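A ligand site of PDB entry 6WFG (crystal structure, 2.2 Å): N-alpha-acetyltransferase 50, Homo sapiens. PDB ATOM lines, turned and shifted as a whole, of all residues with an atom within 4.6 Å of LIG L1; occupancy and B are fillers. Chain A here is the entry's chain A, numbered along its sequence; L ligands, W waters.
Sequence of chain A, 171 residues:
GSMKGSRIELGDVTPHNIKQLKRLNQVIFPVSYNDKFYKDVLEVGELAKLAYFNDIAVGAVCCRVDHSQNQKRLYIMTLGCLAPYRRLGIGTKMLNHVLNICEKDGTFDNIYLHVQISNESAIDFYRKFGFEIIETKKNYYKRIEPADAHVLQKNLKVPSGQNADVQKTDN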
ATOM      1  N   ILE A  28     -22.795  -5.961  -6.922  1.00  0.00           N
ATOM      2  CA  ILE A  28     -22.731  -7.331  -6.430  1.00  0.00           C
ATOM      3  C   ILE A  28     -22.083  -7.416  -5.060  1.00  0.00           C
ATOM      4  O   ILE A  28     -22.610  -8.112  -4.191  1.00  0.00           O
ATOM      5  CB  ILE A  28     -22.029  -8.278  -7.484  1.00  0.00           C
ATOM      6  CG1 ILE A  28     -22.748  -8.247  -8.868  1.00  0.00           C
ATOM      7  CG2 ILE A  28     -21.922  -9.738  -6.957  1.00  0.00           C
ATOM      8  CD1 ILE A  28     -21.869  -8.648 -10.066  1.00  0.00           C
ATOM      9  N   PHE A  29     -20.942  -6.793  -4.870  1.00  0.00           N
ATOM     10  CA  PHE A  29     -20.170  -6.966  -3.660  1.00  0.00           C
ATOM     11  C   PHE A  29     -20.380  -5.883  -2.588  1.00  0.00           C
ATOM     12  O   PHE A  29     -20.601  -4.727  -2.934  1.00  0.00           O
ATOM     13  CB  PHE A  29     -18.668  -7.118  -4.007  1.00  0.00           C
ATOM     14  CG  PHE A  29     -18.472  -8.291  -4.945  1.00  0.00           C
ATOM     15  CD1 PHE A  29     -18.656  -9.592  -4.497  1.00  0.00           C
ATOM     16  CD2 PHE A  29     -18.215  -8.084  -6.303  1.00  0.00           C
ATOM     17  CE1 PHE A  29     -18.518 -10.674  -5.376  1.00  0.00           C
ATOM     18  CE2 PHE A  29     -18.099  -9.161  -7.179  1.00  0.00           C
ATOM     19  CZ  PHE A  29     -18.232 -10.445  -6.709  1.00  0.00           C
ATOM     20  N   MET A  77     -10.246 -12.923  -5.871  1.00  0.00           N
ATOM     21  CA  MET A  77     -10.595 -11.704  -5.139  1.00  0.00           C
ATOM     22  C   MET A  77     -12.091 -11.483  -5.196  1.00  0.00           C
ATOM     23  O   MET A  77     -12.708 -11.151  -4.181  1.00  0.00           O
ATOM     24  CB  MET A  77      -9.854 -10.465  -5.700  1.00  0.00           C
ATOM     25  CG  MET A  77      -8.330 -10.574  -5.659  1.00  0.00           C
ATOM     26  SD  MET A  77      -7.469  -9.147  -6.439  1.00  0.00           S
ATOM     27  CE  MET A  77      -7.827  -9.461  -8.193  1.00  0.00           C
ATOM     28  N   THR A  78     -12.675 -11.610  -6.421  1.00  0.00           N
ATOM     29  CA  THR A  78     -14.110 -11.402  -6.638  1.00  0.00           C
ATOM     30  C   THR A  78     -14.615 -12.392  -7.670  1.00  0.00           C
ATOM     31  O   THR A  78     -13.959 -12.670  -8.677  1.00  0.00           O
ATOM     32  CB  THR A  78     -14.435  -9.939  -7.083  1.00  0.00           C
ATOM     33  OG1 THR A  78     -13.674  -9.599  -8.231  1.00  0.00           O
ATOM     34  CG2 THR A  78     -14.202  -8.902  -6.018  1.00  0.00           C
ATOM     35  N   LEU A  79     -15.784 -12.942  -7.417  1.00  0.00           N
ATOM     36  CA  LEU A  79     -16.454 -13.868  -8.321  1.00  0.00           C
ATOM     37  C   LEU A  79     -17.934 -13.714  -8.028  1.00  0.00           C
ATOM     38  O   LEU A  79     -18.405 -13.991  -6.927  1.00  0.00           O
ATOM     39  CB  LEU A  79     -15.934 -15.334  -8.157  1.00  0.00           C
ATOM     40  CG  LEU A  79     -16.324 -16.338  -9.284  1.00  0.00           C
ATOM     41  CD1 LEU A  79     -15.431 -17.554  -9.240  1.00  0.00           C
ATOM     42  CD2 LEU A  79     -17.773 -16.820  -9.131  1.00  0.00           C
ATOM     43  N   GLY A  80     -18.660 -13.186  -8.987  1.00  0.00           N
ATOM     44  CA  GLY A  80     -20.082 -13.007  -8.746  1.00  0.00           C
ATOM     45  C   GLY A  80     -20.879 -12.590  -9.938  1.00  0.00           C
ATOM     46  O   GLY A  80     -20.341 -12.257 -10.983  1.00  0.00           O
ATOM     47  N   CYS A  81     -22.190 -12.623  -9.770  1.00  0.00           N
ATOM     48  CA  CYS A  81     -23.070 -12.157 -10.813  1.00  0.00           C
ATOM     49  C   CYS A  81     -24.340 -11.524 -10.215  1.00  0.00           C
ATOM     50  O   CYS A  81     -24.618 -11.728  -9.038  1.00  0.00           O
ATOM     51  CB  CYS A  81     -23.347 -13.228 -11.879  1.00  0.00           C
ATOM     52  SG  CYS A  81     -24.752 -14.314 -11.556  1.00  0.00           S
ATOM     53  N   ARG A  86     -28.640 -15.333 -11.095  1.00  0.00           N
ATOM     54  CA  ARG A  86     -28.058 -16.404 -10.281  1.00  0.00           C
ATOM     55  C   ARG A  86     -28.748 -17.734 -10.560  1.00  0.00           C
ATOM     56  O   ARG A  86     -29.906 -17.771 -10.983  1.00  0.00           O
ATOM     57  CB  ARG A  86     -28.033 -16.007  -8.793  1.00  0.00           C
ATOM     58  CG  ARG A  86     -26.997 -14.941  -8.534  1.00  0.00           C
ATOM     59  CD  ARG A  86     -26.952 -14.428  -7.103  1.00  0.00           C
ATOM     60  NE  ARG A  86     -26.160 -13.198  -7.071  1.00  0.00           N
ATOM     61  CZ  ARG A  86     -26.092 -12.348  -6.054  1.00  0.00           C
ATOM     62  NH1 ARG A  86     -26.743 -12.605  -4.930  1.00  0.00           N
ATOM     63  NH2 ARG A  86     -25.370 -11.242  -6.151  1.00  0.00           N
ATOM     64  N   ARG A  87     -28.006 -18.838 -10.344  1.00  0.00           N
ATOM     65  CA  ARG A  87     -28.448 -20.235 -10.519  1.00  0.00           C
ATOM     66  C   ARG A  87     -28.707 -20.605 -11.976  1.00  0.00           C
ATOM     67  O   ARG A  87     -29.564 -21.431 -12.266  1.00  0.00           O
ATOM     68  CB  ARG A  87     -29.658 -20.618  -9.608  1.00  0.00           C
ATOM     69  CG  ARG A  87     -29.486 -20.304  -8.132  1.00  0.00           C
ATOM     70  CD  ARG A  87     -28.383 -21.128  -7.498  1.00  0.00           C
ATOM     71  NE  ARG A  87     -28.711 -22.554  -7.362  1.00  0.00           N
ATOM     72  CZ  ARG A  87     -29.430 -23.058  -6.364  1.00  0.00           C
ATOM     73  NH1 ARG A  87     -29.939 -22.270  -5.432  1.00  0.00           N
ATOM     74  NH2 ARG A  87     -29.645 -24.372  -6.306  1.00  0.00           N
ATOM     75  N   LEU A  88     -27.918 -20.044 -12.898  1.00  0.00           N
ATOM     76  CA  LEU A  88     -28.050 -20.363 -14.328  1.00  0.00           C
ATOM     77  C   LEU A  88     -26.762 -21.007 -14.836  1.00  0.00           C
ATOM     78  O   LEU A  88     -26.671 -21.358 -16.000  1.00  0.00           O
ATOM     79  CB  LEU A  88     -28.366 -19.090 -15.161  1.00  0.00           C
ATOM     80  CG  LEU A  88     -29.767 -18.446 -14.941  1.00  0.00           C
ATOM     81  CD1 LEU A  88     -29.828 -17.094 -15.564  1.00  0.00           C
ATOM     82  CD2 LEU A  88     -30.908 -19.323 -15.500  1.00  0.00           C
ATOM     83  N   GLY A  89     -25.780 -21.150 -13.954  1.00  0.00           N
ATOM     84  CA  GLY A  89     -24.480 -21.707 -14.311  1.00  0.00           C
ATOM     85  C   GLY A  89     -23.405 -20.665 -14.603  1.00  0.00           C
ATOM     86  O   GLY A  89     -22.298 -21.040 -14.982  1.00  0.00           O
ATOM     87  N   ILE A  90     -23.699 -19.358 -14.386  1.00  0.00           N
ATOM     88  CA  ILE A  90     -22.740 -18.254 -14.638  1.00  0.00           C
ATOM     89  C   ILE A  90     -21.530 -18.346 -13.691  1.00  0.00           C
ATOM     90  O   ILE A  90     -20.394 -18.363 -14.164  1.00  0.00           O
ATOM     91  CB  ILE A  90     -23.409 -16.844 -14.654  1.00  0.00           C
ATOM     92  CG1 ILE A  90     -24.501 -16.791 -15.775  1.00  0.00           C
ATOM     93  CG2 ILE A  90     -22.351 -15.717 -14.841  1.00  0.00           C
ATOM     94  CD1 ILE A  90     -25.536 -15.680 -15.657  1.00  0.00           C
ATOM     95  N   GLY A  91     -21.781 -18.534 -12.387  1.00  0.00           N
ATOM     96  CA  GLY A  91     -20.702 -18.736 -11.410  1.00  0.00           C
ATOM     97  C   GLY A  91     -19.825 -19.939 -11.740  1.00  0.00           C
ATOM     98  O   GLY A  91     -18.607 -19.826 -11.700  1.00  0.00           O
ATOM     99  N   THR A  92     -20.450 -21.099 -12.098  1.00  0.00           N
ATOM    100  CA  THR A  92     -19.783 -22.379 -12.492  1.00  0.00           C
ATOM    101  C   THR A  92     -18.879 -22.180 -13.716  1.00  0.00           C
ATOM    102  O   THR A  92     -17.751 -22.672 -13.731  1.00  0.00           O
ATOM    103  CB  THR A  92     -20.863 -23.499 -12.729  1.00  0.00           C
ATOM    104  OG1 THR A  92     -21.427 -23.867 -11.463  1.00  0.00           O
ATOM    105  CG2 THR A  92     -20.301 -24.742 -13.366  1.00  0.00           C
ATOM    106  N   LEU A 113      -9.719 -18.156  -1.296  1.00  0.00           N
ATOM    107  CA  LEU A 113     -10.512 -16.928  -1.295  1.00  0.00           C
ATOM    108  C   LEU A 113     -11.097 -16.666   0.100  1.00  0.00           C
ATOM    109  O   LEU A 113     -11.031 -17.520   0.973  1.00  0.00           O
ATOM    110  CB  LEU A 113     -11.645 -16.987  -2.348  1.00  0.00           C
ATOM    111  CG  LEU A 113     -12.801 -17.975  -2.131  1.00  0.00           C
ATOM    112  CD1 LEU A 113     -14.074 -17.380  -2.605  1.00  0.00           C
ATOM    113  CD2 LEU A 113     -12.571 -19.260  -2.870  1.00  0.00           C
ATOM    114  N   HIS A 114     -11.713 -15.510   0.276  1.00  0.00           N
ATOM    115  CA  HIS A 114     -12.406 -15.155   1.504  1.00  0.00           C
ATOM    116  C   HIS A 114     -13.890 -15.101   1.239  1.00  0.00           C
ATOM    117  O   HIS A 114     -14.330 -14.588   0.200  1.00  0.00           O
ATOM    118  CB  HIS A 114     -11.892 -13.817   2.061  1.00  0.00           C
ATOM    119  CG  HIS A 114     -10.547 -13.911   2.684  1.00  0.00           C
ATOM    120  ND1 HIS A 114      -9.393 -13.710   1.942  1.00  0.00           N
ATOM    121  CD2 HIS A 114     -10.208 -14.145   3.971  1.00  0.00           C
ATOM    122  CE1 HIS A 114      -8.385 -13.847   2.800  1.00  0.00           C
ATOM    123  NE2 HIS A 114      -8.829 -14.139   4.031  1.00  0.00           N
ATOM    124  N   VAL A 115     -14.679 -15.662   2.161  1.00  0.00           N
ATOM    125  CA  VAL A 115     -16.120 -15.657   2.058  1.00  0.00           C
ATOM    126  C   VAL A 115     -16.650 -15.184   3.392  1.00  0.00           C
ATOM    127  O   VAL A 115     -16.508 -15.893   4.392  1.00  0.00           O
ATOM    128  CB  VAL A 115     -16.731 -17.046   1.652  1.00  0.00           C
ATOM    129  CG1 VAL A 115     -18.269 -17.018   1.702  1.00  0.00           C
ATOM    130  CG2 VAL A 115     -16.272 -17.491   0.264  1.00  0.00           C
ATOM    131  N   ASN A 119     -22.573 -15.338   4.118  1.00  0.00           N
ATOM    132  CA  ASN A 119     -22.778 -15.677   2.720  1.00  0.00           C
ATOM    133  C   ASN A 119     -22.831 -17.189   2.533  1.00  0.00           C
ATOM    134  O   ASN A 119     -21.882 -17.836   2.073  1.00  0.00           O
ATOM    135  CB  ASN A 119     -21.732 -14.996   1.841  1.00  0.00           C
ATOM    136  CG  ASN A 119     -22.137 -14.928   0.388  1.00  0.00           C
ATOM    137  OD1 ASN A 119     -23.069 -15.620  -0.058  1.00  0.00           O
ATOM    138  ND2 ASN A 119     -21.367 -14.175  -0.389  1.00  0.00           N
ATOM    139  N   SER A 121     -24.912 -19.057   0.496  1.00  0.00           N
ATOM    140  CA  SER A 121     -24.954 -19.545  -0.878  1.00  0.00           C
ATOM    141  C   SER A 121     -23.558 -19.599  -1.495  1.00  0.00           C
ATOM    142  O   SER A 121     -23.315 -20.470  -2.330  1.00  0.00           O
ATOM    143  CB  SER A 121     -25.932 -18.730  -1.721  1.00  0.00           C
ATOM    144  OG  SER A 121     -25.457 -17.438  -2.027  1.00  0.00           O
ATOM    145  N   ALA A 122     -22.620 -18.719  -1.070  1.00  0.00           N
ATOM    146  CA  ALA A 122     -21.259 -18.765  -1.571  1.00  0.00           C
ATOM    147  C   ALA A 122     -20.520 -19.948  -0.950  1.00  0.00           C
ATOM    148  O   ALA A 122     -19.832 -20.648  -1.672  1.00  0.00           O
ATOM    149  CB  ALA A 122     -20.533 -17.456  -1.304  1.00  0.00           C
ATOM    150  N   ASP A 124     -21.920 -22.829   0.041  1.00  0.00           N
ATOM    151  CA  ASP A 124     -22.560 -23.932  -0.676  1.00  0.00           C
ATOM    152  C   ASP A 124     -21.942 -24.121  -2.063  1.00  0.00           C
ATOM    153  O   ASP A 124     -21.721 -25.253  -2.481  1.00  0.00           O
ATOM    154  CB  ASP A 124     -24.061 -23.639  -0.892  1.00  0.00           C
ATOM    155  CG  ASP A 124     -25.001 -23.949   0.247  1.00  0.00           C
ATOM    156  OD1 ASP A 124     -24.770 -24.963   0.952  1.00  0.00           O
ATOM    157  OD2 ASP A 124     -26.042 -23.268   0.351  1.00  0.00           O
ATOM    158  N   PHE A 125     -21.759 -23.016  -2.785  1.00  0.00           N
ATOM    159  CA  PHE A 125     -21.232 -22.979  -4.142  1.00  0.00           C
ATOM    160  C   PHE A 125     -19.790 -23.504  -4.167  1.00  0.00           C
ATOM    161  O   PHE A 125     -19.492 -24.416  -4.934  1.00  0.00           O
ATOM    162  CB  PHE A 125     -21.314 -21.533  -4.670  1.00  0.00           C
ATOM    163  CG  PHE A 125     -20.668 -21.313  -6.013  1.00  0.00           C
ATOM    164  CD1 PHE A 125     -21.250 -21.811  -7.168  1.00  0.00           C
ATOM    165  CD2 PHE A 125     -19.450 -20.655  -6.112  1.00  0.00           C
ATOM    166  CE1 PHE A 125     -20.634 -21.646  -8.409  1.00  0.00           C
ATOM    167  CE2 PHE A 125     -18.818 -20.505  -7.344  1.00  0.00           C
ATOM    168  CZ  PHE A 125     -19.413 -20.986  -8.488  1.00  0.00           C
ATOM    169  N   TYR A 126     -18.916 -22.948  -3.303  1.00  0.00           N
ATOM    170  CA  TYR A 126     -17.511 -23.332  -3.246  1.00  0.00           C
ATOM    171  C   TYR A 126     -17.309 -24.753  -2.717  1.00  0.00           C
ATOM    172  O   TYR A 126     -16.479 -25.472  -3.254  1.00  0.00           O
ATOM    173  CB  TYR A 126     -16.659 -22.289  -2.502  1.00  0.00           C
ATOM    174  CG  TYR A 126     -16.452 -21.050  -3.353  1.00  0.00           C
ATOM    175  CD1 TYR A 126     -15.590 -21.074  -4.456  1.00  0.00           C
ATOM    176  CD2 TYR A 126     -17.218 -19.905  -3.144  1.00  0.00           C
ATOM    177  CE1 TYR A 126     -15.471 -19.964  -5.292  1.00  0.00           C
ATOM    178  CE2 TYR A 126     -17.066 -18.783  -3.955  1.00  0.00           C
ATOM    179  CZ  TYR A 126     -16.197 -18.814  -5.028  1.00  0.00           C
ATOM    180  OH  TYR A 126     -16.046 -17.726  -5.845  1.00  0.00           O
ATOM    181  N   LYS A 128     -19.240 -27.311  -3.179  1.00  0.00           N
ATOM    182  CA  LYS A 128     -19.680 -28.141  -4.308  1.00  0.00           C
ATOM    183  C   LYS A 128     -18.523 -28.415  -5.274  1.00  0.00           C
ATOM    184  O   LYS A 128     -18.531 -29.416  -6.009  1.00  0.00           O
ATOM    185  CB  LYS A 128     -20.824 -27.421  -5.047  1.00  0.00           C
ATOM    186  CG  LYS A 128     -21.555 -28.249  -6.084  1.00  0.00           C
ATOM    187  CD  LYS A 128     -21.731 -27.444  -7.374  1.00  0.00           C
ATOM    188  CE  LYS A 128     -22.391 -28.234  -8.487  1.00  0.00           C
ATOM    189  NZ  LYS A 128     -23.803 -28.602  -8.178  1.00  0.00           N
HETATM  190  N1  LIG L   1     -28.311 -22.207  -2.398  1.00  0.00           N
HETATM  191  C1  LIG L   1     -27.820 -23.457  -2.476  1.00  0.00           C
HETATM  192  N2  LIG L   1     -26.881 -23.922  -3.310  1.00  0.00           N
HETATM  193  C2  LIG L   1     -26.419 -22.959  -4.117  1.00  0.00           C
HETATM  194  C3  LIG L   1     -26.852 -21.636  -4.136  1.00  0.00           C
HETATM  195  C4  LIG L   1     -27.832 -21.283  -3.234  1.00  0.00           C
HETATM  196  N3  LIG L   1     -28.336 -19.978  -3.200  1.00  0.00           N
HETATM  197  N4  LIG L   1     -26.177 -20.924  -5.098  1.00  0.00           N
HETATM  198  C5  LIG L   1     -25.359 -21.793  -5.649  1.00  0.00           C
HETATM  199  N5  LIG L   1     -25.455 -23.039  -5.086  1.00  0.00           N
HETATM  200  C6  LIG L   1     -24.761 -24.233  -5.554  1.00  0.00           C
HETATM  201  C7  LIG L   1     -25.719 -25.218  -6.208  1.00  0.00           C
HETATM  202  O1  LIG L   1     -25.377 -26.575  -5.980  1.00  0.00           O
HETATM  203  C8  LIG L   1     -25.612 -24.841  -7.665  1.00  0.00           C
HETATM  204  O2  LIG L   1     -25.987 -25.917  -8.513  1.00  0.00           O
HETATM  205  P1  LIG L   1     -27.537 -25.868  -9.052  1.00  0.00           P
HETATM  206  O3  LIG L   1     -27.462 -26.800 -10.233  1.00  0.00           O
HETATM  207  O4  LIG L   1     -28.362 -26.383  -7.897  1.00  0.00           O
HETATM  208  O5  LIG L   1     -27.831 -24.409  -9.379  1.00  0.00           O
HETATM  209  C9  LIG L   1     -24.153 -24.532  -7.801  1.00  0.00           C
HETATM  210  O6  LIG L   1     -23.817 -23.872  -6.578  1.00  0.00           O
HETATM  211  C10 LIG L   1     -23.833 -23.702  -9.041  1.00  0.00           C
HETATM  212  O7  LIG L   1     -24.574 -22.486  -9.127  1.00  0.00           O
HETATM  213  P2  LIG L   1     -24.305 -21.484 -10.379  1.00  0.00           P
HETATM  214  O8  LIG L   1     -25.608 -21.215 -11.077  1.00  0.00           O
HETATM  215  O9  LIG L   1     -23.114 -21.874 -11.215  1.00  0.00           O
HETATM  216  O10 LIG L   1     -23.853 -20.204  -9.481  1.00  0.00           O
HETATM  217  P3  LIG L   1     -24.309 -18.640  -9.533  1.00  0.00           P
HETATM  218  O11 LIG L   1     -24.131 -18.156 -10.950  1.00  0.00           O
HETATM  219  O12 LIG L   1     -25.654 -18.503  -8.851  1.00  0.00           O
HETATM  220  O13 LIG L   1     -23.137 -17.943  -8.665  1.00  0.00           O
HETATM  221  C11 LIG L   1     -22.315 -17.142  -6.520  1.00  0.00           C
HETATM  222  C12 LIG L   1     -22.771 -18.354  -7.332  1.00  0.00           C
HETATM  223  C13 LIG L   1     -21.948 -17.591  -5.123  1.00  0.00           C
HETATM  224  C14 LIG L   1     -21.027 -16.633  -7.141  1.00  0.00           C
HETATM  225  C15 LIG L   1     -23.447 -16.111  -6.552  1.00  0.00           C
HETATM  226  O14 LIG L   1     -24.501 -16.363  -5.616  1.00  0.00           O
HETATM  227  C16 LIG L   1     -23.060 -14.668  -6.374  1.00  0.00           C
HETATM  228  O15 LIG L   1     -22.828 -13.951  -7.336  1.00  0.00           O
HETATM  229  N6  LIG L   1     -23.040 -14.284  -5.057  1.00  0.00           N
HETATM  230  C17 LIG L   1     -22.728 -12.940  -4.625  1.00  0.00           C
HETATM  231  C18 LIG L   1     -21.253 -12.708  -4.735  1.00  0.00           C
HETATM  232  C19 LIG L   1     -20.607 -12.922  -3.411  1.00  0.00           C
HETATM  233  O16 LIG L   1     -20.908 -12.218  -2.449  1.00  0.00           O
HETATM  234  N7  LIG L   1     -19.670 -13.943  -3.455  1.00  0.00           N
HETATM  235  C20 LIG L   1     -18.414 -13.847  -2.727  1.00  0.00           C
HETATM  236  C21 LIG L   1     -17.372 -14.834  -3.215  1.00  0.00           C
HETATM  237  S1  LIG L   1     -15.996 -13.900  -3.965  1.00  0.00           S
HETATM  238  C1  LG2 L   2      -5.061  -9.933  -1.860  1.00  0.00           C
HETATM  239  C2  LG2 L   2      -4.836  -8.638  -2.263  1.00  0.00           C
HETATM  240  C3  LG2 L   2      -3.778 -10.449  -1.508  1.00  0.00           C
HETATM  241  C4  LG2 L   2     -16.884 -11.823   0.051  1.00  0.00           C
HETATM  242  C5  LG2 L   2      -5.733  -7.641  -2.761  1.00  0.00           C
HETATM  243  C6  LG2 L   2     -13.608 -10.848  -0.553  1.00  0.00           C
HETATM  244  C7  LG2 L   2     -12.014  -8.420  -0.050  1.00  0.00           C
HETATM  245  C8  LG2 L   2     -17.449 -10.589  -0.580  1.00  0.00           C
HETATM  246  C9  LG2 L   2     -16.399  -9.691  -1.198  1.00  0.00           C
HETATM  247  C10 LG2 L   2     -15.508 -10.509  -2.099  1.00  0.00           C
HETATM  248  C11 LG2 L   2      -9.107  -7.507  -2.982  1.00  0.00           C
HETATM  249  C12 LG2 L   2      -8.427  -8.818  -1.009  1.00  0.00           C
HETATM  250  C13 LG2 L   2      -7.949  -6.571  -2.716  1.00  0.00           C
HETATM  251  C14 LG2 L   2      -7.301  -7.832  -0.784  1.00  0.00           C
HETATM  252  C15 LG2 L   2     -14.754 -11.518  -1.285  1.00  0.00           C
HETATM  253  C16 LG2 L   2      -9.584  -8.129  -1.691  1.00  0.00           C
HETATM  254  C17 LG2 L   2      -3.297 -12.666  -2.274  1.00  0.00           C
HETATM  255  C18 LG2 L   2      -4.602 -12.397  -0.210  1.00  0.00           C
HETATM  256  C19 LG2 L   2      -2.200 -11.883  -0.216  1.00  0.00           C
HETATM  257  C20 LG2 L   2      -2.734  -7.277  -2.490  1.00  0.00           C
HETATM  258  C21 LG2 L   2     -11.688  -7.076   1.944  1.00  0.00           C
HETATM  259  C22 LG2 L   2     -10.677  -9.124  -2.041  1.00  0.00           C
HETATM  260  C23 LG2 L   2     -11.485  -9.600  -0.842  1.00  0.00           C
HETATM  261  C24 LG2 L   2      -3.468 -11.811  -1.041  1.00  0.00           C
HETATM  262  N1  LG2 L   2      -2.818  -9.552  -1.728  1.00  0.00           N
HETATM  263  N2  LG2 L   2      -3.472  -8.478  -2.157  1.00  0.00           N
HETATM  264  N3  LG2 L   2     -15.585 -12.181  -0.286  1.00  0.00           N
HETATM  265  N4  LG2 L   2      -6.857  -7.259  -2.045  1.00  0.00           N
HETATM  266  N5  LG2 L   2     -12.593 -10.380  -1.354  1.00  0.00           N
HETATM  267  N6  LG2 L   2     -11.341  -8.216   1.144  1.00  0.00           N
HETATM  268  O1  LG2 L   2     -17.589 -12.474   0.819  1.00  0.00           O
HETATM  269  O2  LG2 L   2      -5.475  -7.177  -3.872  1.00  0.00           O
HETATM  270  O3  LG2 L   2     -13.590 -10.713   0.649  1.00  0.00           O
HETATM  271  O4  LG2 L   2     -12.926  -7.701  -0.425  1.00  0.00           O
HETATM  272  O   HOH W   1     -26.009 -18.082 -12.817  1.00  0.00           O
HETATM  273  O   HOH W   2     -26.919 -23.488 -11.758  1.00  0.00           O
HETATM  274  O   HOH W   3     -26.094 -18.392  -6.243  1.00  0.00           O
HETATM  275  O   HOH W   4     -23.944 -15.310  -2.567  1.00  0.00           O
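Residues that only touch LIG L1: Ile 28, Phe 29, Gly 80, Ile 90, Ser 121, Ala 122, Asp 124 and Phe 125. Hydrophobic or aromatic side chains within 4 Å of LIG L1: Ile 28, Phe 29, Leu 79, Ile 90 and Phe 125. Of the 24 residues printed, 18 come within 4 Å of LIG L1. Along chain A the residues within 4 Å of LIG L1 span positions 28 to 128.
N of Arg 87 is in hydrogen-bond range of O12 of LIG L1 (2.8 Å). An oxygen (O8) of LIG L1 lies within hydrogen-bond range of the backbone NH (N) of Gly 89, 2.9 Å away. An oxygen (O15) of LIG L1 sits at hydrogen-bond distance from the backbone NH (N) of Cys 81 (2.8 Å). The backbone carbonyl oxygen (O) of His 114 sits at hydrogen-bond distance from a nitrogen (N3) of LG2 L2, at 2.8 Å. O9 of LIG L1 lies within hydrogen-bond range of OG1 of Thr 92 (2.6 Å). O4 of LIG L1 lies within salt-bridge range of NH2 of Arg 87 (2.9 Å). O of Met 77 lies within hydrogen-bond range of N5 of LG2 L2, 2.9 Å away. An oxygen (O9) of LIG L1 is in hydrogen-bond range of the backbone NH (N) of Thr 92, at 2.9 Å. The backbone NH (N) of Leu 88 lies within hydrogen-bond range of an oxygen (O8) of LIG L1. The guanidinium group (NE) of Arg 86 sits at hydrogen-bond distance from an oxygen (O15) of LIG L1, at 3.4 Å. NZ of Lys 128 is in hydrogen-bond range of O1 of LIG L1 (3.4 Å). The backbone NH (N) of Leu 79 lies close to a sulfur (S1) of LIG L1, 3.6 Å away. The backbone NH of Gly 91 lies within hydrogen-bond range of an oxygen (O11) of LIG L1, at 2.8 Å. O16 of LIG L1 is in hydrogen-bond range of ND2 of Asn 119, 2.9 Å away.
Water W2 lies within hydrogen-bond range of O5 of LIG L1, O of Arg 87 and N of Gly 89. Water W4 lies within hydrogen-bond range of OG of Ser 121 (2.7 Å), OD1 of Asn 119 (2.7 Å) and N6 of LIG L1 (2.8 Å).
NE of Arg 86 lies within hydrogen-bond range of O of Cys 81 (2.9 Å). N of Ala 122 is in hydrogen-bond range of OD1 of Asn 119, 3.3 Å away.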
